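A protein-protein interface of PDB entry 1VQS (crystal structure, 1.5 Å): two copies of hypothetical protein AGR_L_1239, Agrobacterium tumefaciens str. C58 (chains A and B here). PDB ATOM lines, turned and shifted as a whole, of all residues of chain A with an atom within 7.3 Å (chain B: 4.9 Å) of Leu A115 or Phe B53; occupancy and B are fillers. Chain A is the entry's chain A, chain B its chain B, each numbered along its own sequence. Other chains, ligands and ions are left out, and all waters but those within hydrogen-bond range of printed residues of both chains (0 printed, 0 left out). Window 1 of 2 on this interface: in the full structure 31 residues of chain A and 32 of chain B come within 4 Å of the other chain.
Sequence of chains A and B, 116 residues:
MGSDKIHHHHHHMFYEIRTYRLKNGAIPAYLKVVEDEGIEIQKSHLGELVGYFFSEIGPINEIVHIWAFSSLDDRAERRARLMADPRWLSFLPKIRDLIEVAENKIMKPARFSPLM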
ATOM      1  N   HIS A  12      36.168  -6.202  30.640  1.00  0.00           N
ATOM      2  CA  HIS A  12      34.700  -6.280  30.638  1.00  0.00           C
ATOM      3  C   HIS A  12      34.320  -7.715  30.261  1.00  0.00           C
ATOM      4  O   HIS A  12      35.134  -8.439  29.680  1.00  0.00           O
ATOM      5  CB  HIS A  12      34.135  -5.305  29.592  1.00  0.00           C
ATOM      6  CG  HIS A  12      34.371  -5.763  28.197  1.00  0.00           C
ATOM      7  ND1 HIS A  12      33.534  -6.663  27.566  1.00  0.00           N
ATOM      8  CD2 HIS A  12      35.404  -5.545  27.348  1.00  0.00           C
ATOM      9  CE1 HIS A  12      34.020  -6.940  26.367  1.00  0.00           C
ATOM     10  NE2 HIS A  12      35.153  -6.275  26.210  1.00  0.00           N
ATOM     11  N   MET A  13      33.098  -8.124  30.578  1.00  0.00           N
ATOM     12  CA  MET A  13      32.591  -9.420  30.148  1.00  0.00           C
ATOM     13  C   MET A  13      31.870  -9.247  28.811  1.00  0.00           C
ATOM     14  O   MET A  13      31.490  -8.134  28.450  1.00  0.00           O
ATOM     15  CB  MET A  13      31.614  -9.983  31.194  1.00  0.00           C
ATOM     16  CG  MET A  13      32.169 -10.125  32.610  1.00  0.00           C
ATOM     17  SD  MET A  13      33.558 -11.511  32.771  1.00  0.00           S
ATOM     18  CE  MET A  13      32.416 -13.075  32.860  1.00  0.00           C
ATOM     19  N   PHE A  14      31.720 -10.355  28.089  1.00  0.00           N
ATOM     20  CA  PHE A  14      30.807 -10.494  26.948  1.00  0.00           C
ATOM     21  C   PHE A  14      29.482 -11.062  27.440  1.00  0.00           C
ATOM     22  O   PHE A  14      29.488 -12.014  28.238  1.00  0.00           O
ATOM     23  CB  PHE A  14      31.393 -11.462  25.944  1.00  0.00           C
ATOM     24  CG  PHE A  14      32.597 -10.928  25.255  1.00  0.00           C
ATOM     25  CD1 PHE A  14      33.850 -11.117  25.793  1.00  0.00           C
ATOM     26  CD2 PHE A  14      32.480 -10.221  24.073  1.00  0.00           C
ATOM     27  CE1 PHE A  14      34.969 -10.618  25.172  1.00  0.00           C
ATOM     28  CE2 PHE A  14      33.620  -9.709  23.432  1.00  0.00           C
ATOM     29  CZ  PHE A  14      34.846  -9.885  23.994  1.00  0.00           C
ATOM     30  N   TYR A  15      28.364 -10.529  26.942  1.00  0.00           N
ATOM     31  CA  TYR A  15      27.038 -10.967  27.320  1.00  0.00           C
ATOM     32  C   TYR A  15      26.383 -11.682  26.177  1.00  0.00           C
ATOM     33  O   TYR A  15      26.161 -11.073  25.123  1.00  0.00           O
ATOM     34  CB  TYR A  15      26.197  -9.768  27.777  1.00  0.00           C
ATOM     35  CG  TYR A  15      26.706  -9.308  29.131  1.00  0.00           C
ATOM     36  CD1 TYR A  15      27.817  -8.502  29.244  1.00  0.00           C
ATOM     37  CD2 TYR A  15      26.109  -9.743  30.316  1.00  0.00           C
ATOM     38  CE1 TYR A  15      28.330  -8.135  30.507  1.00  0.00           C
ATOM     39  CE2 TYR A  15      26.599  -9.361  31.558  1.00  0.00           C
ATOM     40  CZ  TYR A  15      27.717  -8.579  31.645  1.00  0.00           C
ATOM     41  OH  TYR A  15      28.180  -8.227  32.927  1.00  0.00           O
ATOM     42  N   ILE A  17      23.008 -13.169  24.793  1.00  0.00           N
ATOM     43  CA  ILE A  17      21.545 -13.117  24.991  1.00  0.00           C
ATOM     44  C   ILE A  17      20.917 -14.171  24.089  1.00  0.00           C
ATOM     45  O   ILE A  17      21.089 -14.122  22.866  1.00  0.00           O
ATOM     46  CB  ILE A  17      20.942 -11.708  24.742  1.00  0.00           C
ATOM     47  CG1 ILE A  17      21.621 -10.687  25.675  1.00  0.00           C
ATOM     48  CG2 ILE A  17      19.408 -11.726  24.960  1.00  0.00           C
ATOM     49  CD1 ILE A  17      21.110  -9.246  25.484  1.00  0.00           C
ATOM     50  N   GLU A  48      28.579 -18.060  34.598  1.00  0.00           N
ATOM     51  CA  GLU A  48      27.901 -16.853  35.096  1.00  0.00           C
ATOM     52  C   GLU A  48      26.565 -16.632  34.402  1.00  0.00           C
ATOM     53  O   GLU A  48      26.467 -15.880  33.403  1.00  0.00           O
ATOM     54  CB  GLU A  48      28.764 -15.581  34.970  1.00  0.00           C
ATOM     55  CG  GLU A  48      28.134 -14.431  35.760  1.00  0.00           C
ATOM     56  CD  GLU A  48      28.868 -13.095  35.683  1.00  0.00           C
ATOM     57  OE1 GLU A  48      30.091 -13.066  35.462  1.00  0.00           O
ATOM     58  OE2 GLU A  48      28.186 -12.053  35.847  1.00  0.00           O
ATOM     59  N   VAL A  50      23.365 -14.644  34.238  1.00  0.00           N
ATOM     60  CA  VAL A  50      23.065 -13.261  34.556  1.00  0.00           C
ATOM     61  C   VAL A  50      21.587 -13.098  34.871  1.00  0.00           C
ATOM     62  O   VAL A  50      21.226 -12.495  35.874  1.00  0.00           O
ATOM     63  CB  VAL A  50      23.498 -12.362  33.380  1.00  0.00           C
ATOM     64  CG1 VAL A  50      23.004 -10.918  33.567  1.00  0.00           C
ATOM     65  CG2 VAL A  50      25.026 -12.422  33.229  1.00  0.00           C
ATOM     66  N   GLY A  51      20.729 -13.595  33.984  1.00  0.00           N
ATOM     67  CA  GLY A  51      19.287 -13.436  34.154  1.00  0.00           C
ATOM     68  C   GLY A  51      18.548 -14.457  33.303  1.00  0.00           C
ATOM     69  O   GLY A  51      19.085 -14.969  32.328  1.00  0.00           O
ATOM     70  N   ILE A  66      20.473 -14.858  29.750  1.00  0.00           N
ATOM     71  CA  ILE A  66      21.667 -14.086  29.545  1.00  0.00           C
ATOM     72  C   ILE A  66      22.768 -14.700  30.351  1.00  0.00           C
ATOM     73  O   ILE A  66      22.576 -14.999  31.525  1.00  0.00           O
ATOM     74  CB  ILE A  66      21.447 -12.640  29.992  1.00  0.00           C
ATOM     75  CG1 ILE A  66      20.239 -12.021  29.282  1.00  0.00           C
ATOM     76  CG2 ILE A  66      22.727 -11.831  29.716  1.00  0.00           C
ATOM     77  CD1 ILE A  66      19.932 -10.573  29.659  1.00  0.00           C
ATOM     78  N   ALA A  68      27.209 -14.403  31.029  1.00  0.00           N
ATOM     79  CA  ALA A  68      28.421 -13.578  30.889  1.00  0.00           C
ATOM     80  C   ALA A  68      29.649 -14.469  30.745  1.00  0.00           C
ATOM     81  O   ALA A  68      29.781 -15.465  31.471  1.00  0.00           O
ATOM     82  CB  ALA A  68      28.596 -12.662  32.094  1.00  0.00           C
ATOM     83  N   ILE A 106      25.797 -11.844  20.818  1.00  0.00           N
ATOM     84  CA  ILE A 106      26.794 -11.429  21.780  1.00  0.00           C
ATOM     85  C   ILE A 106      26.767  -9.922  21.821  1.00  0.00           C
ATOM     86  O   ILE A 106      26.823  -9.277  20.759  1.00  0.00           O
ATOM     87  CB  ILE A 106      28.209 -11.854  21.384  1.00  0.00           C
ATOM     88  CG1 ILE A 106      28.309 -13.372  21.286  1.00  0.00           C
ATOM     89  CG2 ILE A 106      29.257 -11.273  22.375  1.00  0.00           C
ATOM     90  CD1 ILE A 106      28.009 -14.127  22.542  1.00  0.00           C
ATOM     91  N   MET A 107      26.702  -9.362  23.024  1.00  0.00           N
ATOM     92  CA  MET A 107      26.713  -7.945  23.175  1.00  0.00           C
ATOM     93  C   MET A 107      27.814  -7.560  24.216  1.00  0.00           C
ATOM     94  O   MET A 107      28.332  -8.387  24.954  1.00  0.00           O
ATOM     95  CB  MET A 107      25.237  -7.435  23.445  1.00  0.00           C
ATOM     96  CG  MET A 107      23.968  -7.699  22.227  1.00  0.00           C
ATOM     97  SD  MET A 107      22.643  -6.862  22.901  1.00  0.00           S
ATOM     98  CE  MET A 107      23.007  -5.217  22.082  1.00  0.00           C
ATOM     99  N   LYS A 108      28.233  -6.303  24.196  1.00  0.00           N
ATOM    100  CA  LYS A 108      29.230  -5.780  25.121  1.00  0.00           C
ATOM    101  C   LYS A 108      28.589  -4.729  26.008  1.00  0.00           C
ATOM    102  O   LYS A 108      27.637  -4.081  25.597  1.00  0.00           O
ATOM    103  CB  LYS A 108      30.396  -5.145  24.363  1.00  0.00           C
ATOM    104  CG  LYS A 108      31.189  -6.161  23.590  1.00  0.00           C
ATOM    105  CD  LYS A 108      32.211  -5.522  22.649  1.00  0.00           C
ATOM    106  CE  LYS A 108      33.568  -5.436  23.237  1.00  0.00           C
ATOM    107  NZ  LYS A 108      34.556  -4.998  22.185  1.00  0.00           N
ATOM    108  N   PRO A 109      29.078  -4.591  27.260  1.00  0.00           N
ATOM    109  CA  PRO A 109      28.532  -3.591  28.156  1.00  0.00           C
ATOM    110  C   PRO A 109      29.020  -2.178  27.850  1.00  0.00           C
ATOM    111  O   PRO A 109      30.213  -1.971  27.587  1.00  0.00           O
ATOM    112  CB  PRO A 109      29.037  -4.048  29.520  1.00  0.00           C
ATOM    113  CG  PRO A 109      30.344  -4.679  29.223  1.00  0.00           C
ATOM    114  CD  PRO A 109      30.130  -5.387  27.912  1.00  0.00           C
ATOM    115  N   ALA A 110      28.094  -1.212  27.855  1.00  0.00           N
ATOM    116  CA  ALA A 110      28.493   0.188  27.895  1.00  0.00           C
ATOM    117  C   ALA A 110      29.296   0.486  29.161  1.00  0.00           C
ATOM    118  O   ALA A 110      29.198  -0.232  30.148  1.00  0.00           O
ATOM    119  CB  ALA A 110      27.262   1.074  27.856  1.00  0.00           C
ATOM    120  N   ARG A 111      30.072   1.565  29.143  1.00  0.00           N
ATOM    121  CA  ARG A 111      30.898   1.907  30.301  1.00  0.00           C
ATOM    122  C   ARG A 111      30.062   2.163  31.541  1.00  0.00           C
ATOM    123  O   ARG A 111      30.544   1.997  32.672  1.00  0.00           O
ATOM    124  CB  ARG A 111      31.724   3.149  29.993  1.00  0.00           C
ATOM    125  CG  ARG A 111      32.819   2.877  28.998  1.00  0.00           C
ATOM    126  CD  ARG A 111      33.394   4.126  28.321  1.00  0.00           C
ATOM    127  NE  ARG A 111      33.535   5.235  29.252  1.00  0.00           N
ATOM    128  CZ  ARG A 111      34.518   5.376  30.134  1.00  0.00           C
ATOM    129  NH1 ARG A 111      35.498   4.480  30.226  1.00  0.00           N
ATOM    130  NH2 ARG A 111      34.517   6.437  30.934  1.00  0.00           N
ATOM    131  N   PHE A 112      28.812   2.568  31.346  1.00  0.00           N
ATOM    132  CA  PHE A 112      27.911   2.892  32.444  1.00  0.00           C
ATOM    133  C   PHE A 112      26.908   1.766  32.745  1.00  0.00           C
ATOM    134  O   PHE A 112      25.946   1.954  33.493  1.00  0.00           O
ATOM    135  CB  PHE A 112      27.198   4.226  32.142  1.00  0.00           C
ATOM    136  CG  PHE A 112      26.623   4.300  30.750  1.00  0.00           C
ATOM    137  CD1 PHE A 112      25.341   3.840  30.482  1.00  0.00           C
ATOM    138  CD2 PHE A 112      27.358   4.787  29.689  1.00  0.00           C
ATOM    139  CE1 PHE A 112      24.811   3.909  29.223  1.00  0.00           C
ATOM    140  CE2 PHE A 112      26.836   4.826  28.408  1.00  0.00           C
ATOM    141  CZ  PHE A 112      25.550   4.381  28.169  1.00  0.00           C
ATOM    142  N   SER A 113      27.125   0.579  32.176  1.00  0.00           N
ATOM    143  CA  SER A 113      26.291  -0.549  32.534  1.00  0.00           C
ATOM    144  C   SER A 113      26.666  -1.076  33.923  1.00  0.00           C
ATOM    145  O   SER A 113      27.856  -1.269  34.217  1.00  0.00           O
ATOM    146  CB  SER A 113      26.497  -1.673  31.522  1.00  0.00           C
ATOM    147  OG  SER A 113      25.685  -2.797  31.861  1.00  0.00           O
ATOM    148  N   PRO A 114      25.663  -1.289  34.802  1.00  0.00           N
ATOM    149  CA  PRO A 114      25.958  -1.936  36.078  1.00  0.00           C
ATOM    150  C   PRO A 114      26.454  -3.370  35.923  1.00  0.00           C
ATOM    151  O   PRO A 114      27.118  -3.874  36.829  1.00  0.00           O
ATOM    152  CB  PRO A 114      24.621  -1.905  36.809  1.00  0.00           C
ATOM    153  CG  PRO A 114      23.876  -0.770  36.177  1.00  0.00           C
ATOM    154  CD  PRO A 114      24.264  -0.839  34.741  1.00  0.00           C
ATOM    155  N   LEU A 115      26.100  -4.027  34.818  1.00  0.00           N
ATOM    156  CA  LEU A 115      26.642  -5.330  34.466  1.00  0.00           C
ATOM    157  C   LEU A 115      27.806  -5.065  33.531  1.00  0.00           C
ATOM    158  O   LEU A 115      27.621  -4.574  32.404  1.00  0.00           O
ATOM    159  CB  LEU A 115      25.565  -6.175  33.778  1.00  0.00           C
ATOM    160  CG  LEU A 115      24.452  -6.760  34.667  1.00  0.00           C
ATOM    161  CD1 LEU A 115      23.338  -7.283  33.836  1.00  0.00           C
ATOM    162  CD2 LEU A 115      24.996  -7.860  35.567  1.00  0.00           C
ATOM    163  N   MET A 116      29.013  -5.336  34.012  1.00  0.00           N
ATOM    164  CA  MET A 116      30.219  -4.898  33.338  1.00  0.00           C
ATOM    165  C   MET A 116      30.926  -6.093  32.725  1.00  0.00           C
ATOM    166  O   MET A 116      30.525  -7.256  32.888  1.00  0.00           O
ATOM    167  OXT MET A 116      31.940  -5.897  32.065  1.00  0.00           O
ATOM    168  CB  MET A 116      31.148  -4.139  34.325  1.00  0.00           C
ATOM    169  CG  MET A 116      30.647  -2.656  34.453  1.00  0.00           C
ATOM    170  SD  MET A 116      30.412  -1.697  32.623  1.00  0.00           S
ATOM    171  CE  MET A 116      32.120  -2.331  31.861  1.00  0.00           C
ATOM    172  N   VAL B  50      19.511  -2.129  35.085  1.00  0.00           N
ATOM    173  CA  VAL B  50      20.028  -3.493  35.232  1.00  0.00           C
ATOM    174  C   VAL B  50      21.255  -3.715  34.351  1.00  0.00           C
ATOM    175  O   VAL B  50      22.282  -4.225  34.803  1.00  0.00           O
ATOM    176  CB  VAL B  50      18.920  -4.502  34.891  1.00  0.00           C
ATOM    177  CG1 VAL B  50      19.470  -5.898  34.834  1.00  0.00           C
ATOM    178  CG2 VAL B  50      17.798  -4.437  35.929  1.00  0.00           C
ATOM    179  N   GLY B  51      21.147  -3.317  33.102  1.00  0.00           N
ATOM    180  CA  GLY B  51      22.254  -3.498  32.185  1.00  0.00           C
ATOM    181  C   GLY B  51      22.071  -2.629  30.957  1.00  0.00           C
ATOM    182  O   GLY B  51      20.957  -2.216  30.645  1.00  0.00           O
ATOM    183  N   TYR B  52      23.174  -2.320  30.285  1.00  0.00           N
ATOM    184  CA  TYR B  52      23.138  -1.435  29.136  1.00  0.00           C
ATOM    185  C   TYR B  52      24.206  -1.925  28.168  1.00  0.00           C
ATOM    186  O   TYR B  52      25.389  -1.858  28.475  1.00  0.00           O
ATOM    187  CB  TYR B  52      23.403  -0.001  29.585  1.00  0.00           C
ATOM    188  CG  TYR B  52      22.749   1.070  28.702  1.00  0.00           C
ATOM    189  CD1 TYR B  52      23.151   1.271  27.388  1.00  0.00           C
ATOM    190  CD2 TYR B  52      21.768   1.917  29.219  1.00  0.00           C
ATOM    191  CE1 TYR B  52      22.552   2.260  26.582  1.00  0.00           C
ATOM    192  CE2 TYR B  52      21.168   2.905  28.420  1.00  0.00           C
ATOM    193  CZ  TYR B  52      21.568   3.071  27.101  1.00  0.00           C
ATOM    194  OH  TYR B  52      21.002   4.062  26.283  1.00  0.00           O
ATOM    195  N   PHE B  53      23.786  -2.394  26.990  1.00  0.00           N
ATOM    196  CA  PHE B  53      24.650  -3.159  26.086  1.00  0.00           C
ATOM    197  C   PHE B  53      24.579  -2.633  24.664  1.00  0.00           C
ATOM    198  O   PHE B  53      23.601  -2.030  24.257  1.00  0.00           O
ATOM    199  CB  PHE B  53      24.234  -4.637  26.055  1.00  0.00           C
ATOM    200  CG  PHE B  53      24.036  -5.237  27.425  1.00  0.00           C
ATOM    201  CD1 PHE B  53      25.119  -5.601  28.181  1.00  0.00           C
ATOM    202  CD2 PHE B  53      22.778  -5.422  27.969  1.00  0.00           C
ATOM    203  CE1 PHE B  53      24.966  -6.154  29.445  1.00  0.00           C
ATOM    204  CE2 PHE B  53      22.630  -5.977  29.266  1.00  0.00           C
ATOM    205  CZ  PHE B  53      23.727  -6.346  29.976  1.00  0.00           C
ATOM    206  N   PHE B  54      25.639  -2.919  23.928  1.00  0.00           N
ATOM    207  CA  PHE B  54      25.692  -2.634  22.500  1.00  0.00           C
ATOM    208  C   PHE B  54      26.170  -3.861  21.739  1.00  0.00           C
ATOM    209  O   PHE B  54      26.811  -4.743  22.289  1.00  0.00           O
ATOM    210  CB  PHE B  54      26.561  -1.413  22.174  1.00  0.00           C
ATOM    211  CG  PHE B  54      27.987  -1.541  22.556  1.00  0.00           C
ATOM    212  CD1 PHE B  54      28.409  -1.262  23.850  1.00  0.00           C
ATOM    213  CD2 PHE B  54      28.931  -1.906  21.614  1.00  0.00           C
ATOM    214  CE1 PHE B  54      29.738  -1.351  24.179  1.00  0.00           C
ATOM    215  CE2 PHE B  54      30.264  -2.013  21.941  1.00  0.00           C
ATOM    216  CZ  PHE B  54      30.665  -1.742  23.223  1.00  0.00           C
ATOM    217  N   SER B  55      25.758  -3.982  20.479  1.00  0.00           N
ATOM    218  CA  SER B  55      25.945  -5.256  19.798  1.00  0.00           C
ATOM    219  C   SER B  55      27.368  -5.482  19.261  1.00  0.00           C
ATOM    220  O   SER B  55      28.046  -4.550  18.845  1.00  0.00           O
ATOM    221  CB  SER B  55      24.863  -5.483  18.724  1.00  0.00           C
ATOM    222  OG  SER B  55      24.684  -4.399  17.843  1.00  0.00           O
ATOM    223  N   GLU B  62      22.985  -2.129  17.307  1.00  0.00           N
ATOM    224  CA  GLU B  62      21.919  -2.340  18.279  1.00  0.00           C
ATOM    225  C   GLU B  62      22.324  -1.943  19.692  1.00  0.00           C
ATOM    226  O   GLU B  62      23.438  -2.220  20.152  1.00  0.00           O
ATOM    227  CB  GLU B  62      21.461  -3.794  18.266  1.00  0.00           C
ATOM    228  CG  GLU B  62      20.219  -4.072  19.108  1.00  0.00           C
ATOM    229  CD  GLU B  62      19.750  -5.508  19.012  1.00  0.00           C
ATOM    230  OE1 GLU B  62      20.322  -6.357  19.744  1.00  0.00           O
ATOM    231  OE2 GLU B  62      18.833  -5.743  18.214  1.00  0.00           O
ATOM    232  N   ILE B  63      21.381  -1.307  20.379  1.00  0.00           N
ATOM    233  CA  ILE B  63      21.443  -1.004  21.816  1.00  0.00           C
ATOM    234  C   ILE B  63      20.369  -1.825  22.538  1.00  0.00           C
ATOM    235  O   ILE B  63      19.235  -1.877  22.069  1.00  0.00           O
ATOM    236  CB  ILE B  63      21.221   0.495  22.076  1.00  0.00           C
ATOM    237  CG1 ILE B  63      22.354   1.326  21.457  1.00  0.00           C
ATOM    238  CG2 ILE B  63      21.115   0.799  23.588  1.00  0.00           C
ATOM    239  CD1 ILE B  63      23.714   1.127  22.053  1.00  0.00           C
ATOM    240  N   VAL B  64      20.709  -2.453  23.663  1.00  0.00           N
ATOM    241  CA  VAL B  64      19.716  -3.073  24.534  1.00  0.00           C
ATOM    242  C   VAL B  64      19.932  -2.569  25.932  1.00  0.00           C
ATOM    243  O   VAL B  64      21.046  -2.625  26.439  1.00  0.00           O
ATOM    244  CB  VAL B  64      19.849  -4.569  24.544  1.00  0.00           C
ATOM    245  CG1 VAL B  64      18.978  -5.200  25.660  1.00  0.00           C
ATOM    246  CG2 VAL B  64      19.454  -5.157  23.205  1.00  0.00           C
ATOM    247  N   ILE B  66      18.087  -2.558  29.985  1.00  0.00           N
ATOM    248  CA  ILE B  66      17.173  -3.276  30.822  1.00  0.00           C
ATOM    249  C   ILE B  66      17.007  -2.537  32.140  1.00  0.00           C
ATOM    250  O   ILE B  66      17.993  -2.121  32.772  1.00  0.00           O
ATOM    251  CB  ILE B  66      17.709  -4.657  31.108  1.00  0.00           C
ATOM    252  CG1 ILE B  66      18.043  -5.375  29.804  1.00  0.00           C
ATOM    253  CG2 ILE B  66      16.725  -5.410  31.954  1.00  0.00           C
ATOM    254  CD1 ILE B  66      18.486  -6.802  29.978  1.00  0.00           C
ATOM    255  N   LEU B 115      18.682 -12.369  38.695  1.00  0.00           N
ATOM    256  CA  LEU B 115      17.960 -11.100  38.655  1.00  0.00           C
ATOM    257  C   LEU B 115      16.529 -11.464  38.998  1.00  0.00           C
ATOM    258  O   LEU B 115      15.818 -12.082  38.180  1.00  0.00           O
ATOM    259  CB  LEU B 115      18.071 -10.433  37.285  1.00  0.00           C
ATOM    260  CG  LEU B 115      19.453  -9.855  37.046  1.00  0.00           C
ATOM    261  CD1 LEU B 115      19.655  -9.553  35.574  1.00  0.00           C
ATOM    262  CD2 LEU B 115      19.677  -8.601  37.906  1.00  0.00           C
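The backbone NH of Lys A108 lies within hydrogen-bond range of the backbone carbonyl oxygen of Phe B54.
The backbone NH of Ala A110 is in hydrogen-bond range of the backbone carbonyl oxygen of Tyr B52, at 2.8 Å.
N of Tyr B52 sits at hydrogen-bond distance from OG of Ser A113, at 3.0 Å.
The side-chain hydroxyl of Tyr A15 lies within hydrogen-bond range of the chain-end carboxylate of Met A116 (2.5 Å).
The backbone NH (N) of Val A50 lies within hydrogen-bond range of the backbone carbonyl oxygen (O) of Ile A66.
The backbone carbonyl oxygen of Tyr A15 is in hydrogen-bond range of the backbone NH of Met A107.
The backbone NH of Glu B62 lies within hydrogen-bond range of the side-chain hydroxyl of Ser B55, at 2.9 Å.
The side-chain hydroxyl (OG) of Ser A113 is in hydrogen-bond range of the backbone carbonyl oxygen (O) of Leu A115 (2.7 Å).
N of Phe B53 lies within hydrogen-bond range of O of Val B64, 2.8 Å away.
Tyr A15 touches Phe B53.
Met A107 touches Phe B53.
CE of Met A107 touches N of Ser B55, at 3.4 Å.
O of Glu B62 touches CE of Met A107, 3.6 Å away.
Met A107 touches Val B64 (SD to CG2, 3.6 Å).
Phe B54 touches Pro A109 (CE1 to O, 3.5 Å).
Phe A112 touches Tyr B52.
CB of Pro A114 touches O of Val B50, at 3.9 Å.
CG of Leu A115 touches O of Val B50 (3.3 Å).
Phe B53 touches Leu A115.
Of the printed residues of chain B, Leu A115 touches Val B50 (3.3 Å) and Phe B53 (3.99 Å).
Of the printed residues of chain A, Phe B53 touches Tyr A15 (3.6 Å), Met A107 (3.9 Å), Lys A108 (3.2 Å), Pro A109 (3.96 Å) and Leu A115 (3.99 Å).
Of the printed residues of chain B, Met A107 touches Phe B53, Phe B54, Ser B55, Glu B62 and Val B64.
Of the printed residues of chain B, Pro A109 touches Tyr B52 (3.6 Å), Phe B53 (3.96 Å) and Phe B54 (3.5 Å).
Of the printed residues of chain A, Val B50 touches Pro A114 (3.9 Å) and Leu A115 (3.3 Å).
Printed residues of chain A within 4 Å of Tyr B52: Pro A109 (3.6 Å), Ala A110 (2.8 Å), Phe A112 (3.5 Å) and Ser A113 (3.0 Å).
Printed residues of chain A within 4 Å of Glu B62: Met A107 (3.6 Å).
Ile A66 touches none of the printed residues of chain B.
The nearest printed residue of chain A that does not touch Phe B53 is Ser A113 (4.2 Å).
The nearest printed residue of chain A that does not touch Leu B115 is Gly A51 (4.2 Å).
Hydrophobic or aromatic side chains of chain B within 4 Å of the printed part of chain A: Tyr B52, Phe B53, Phe B54, Val B64 and Leu B115.
Hydrophobic or aromatic side chains of chain A that line the printed part of chain B: Tyr A15, Met A107, Ala A110, Phe A112, Pro A114 and Leu A115.
Among the printed residues, 19 pairs touch across the chains.
Val A50 touches Leu B115, and with the chains exchanged Leu A115 touches Val B50.
Positions printed for both chains: 50, 51, 66 and 115.
Of the 19 pairs that touch across the chains among the printed residues, 2 have their exchanged pair printed and touching as well.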
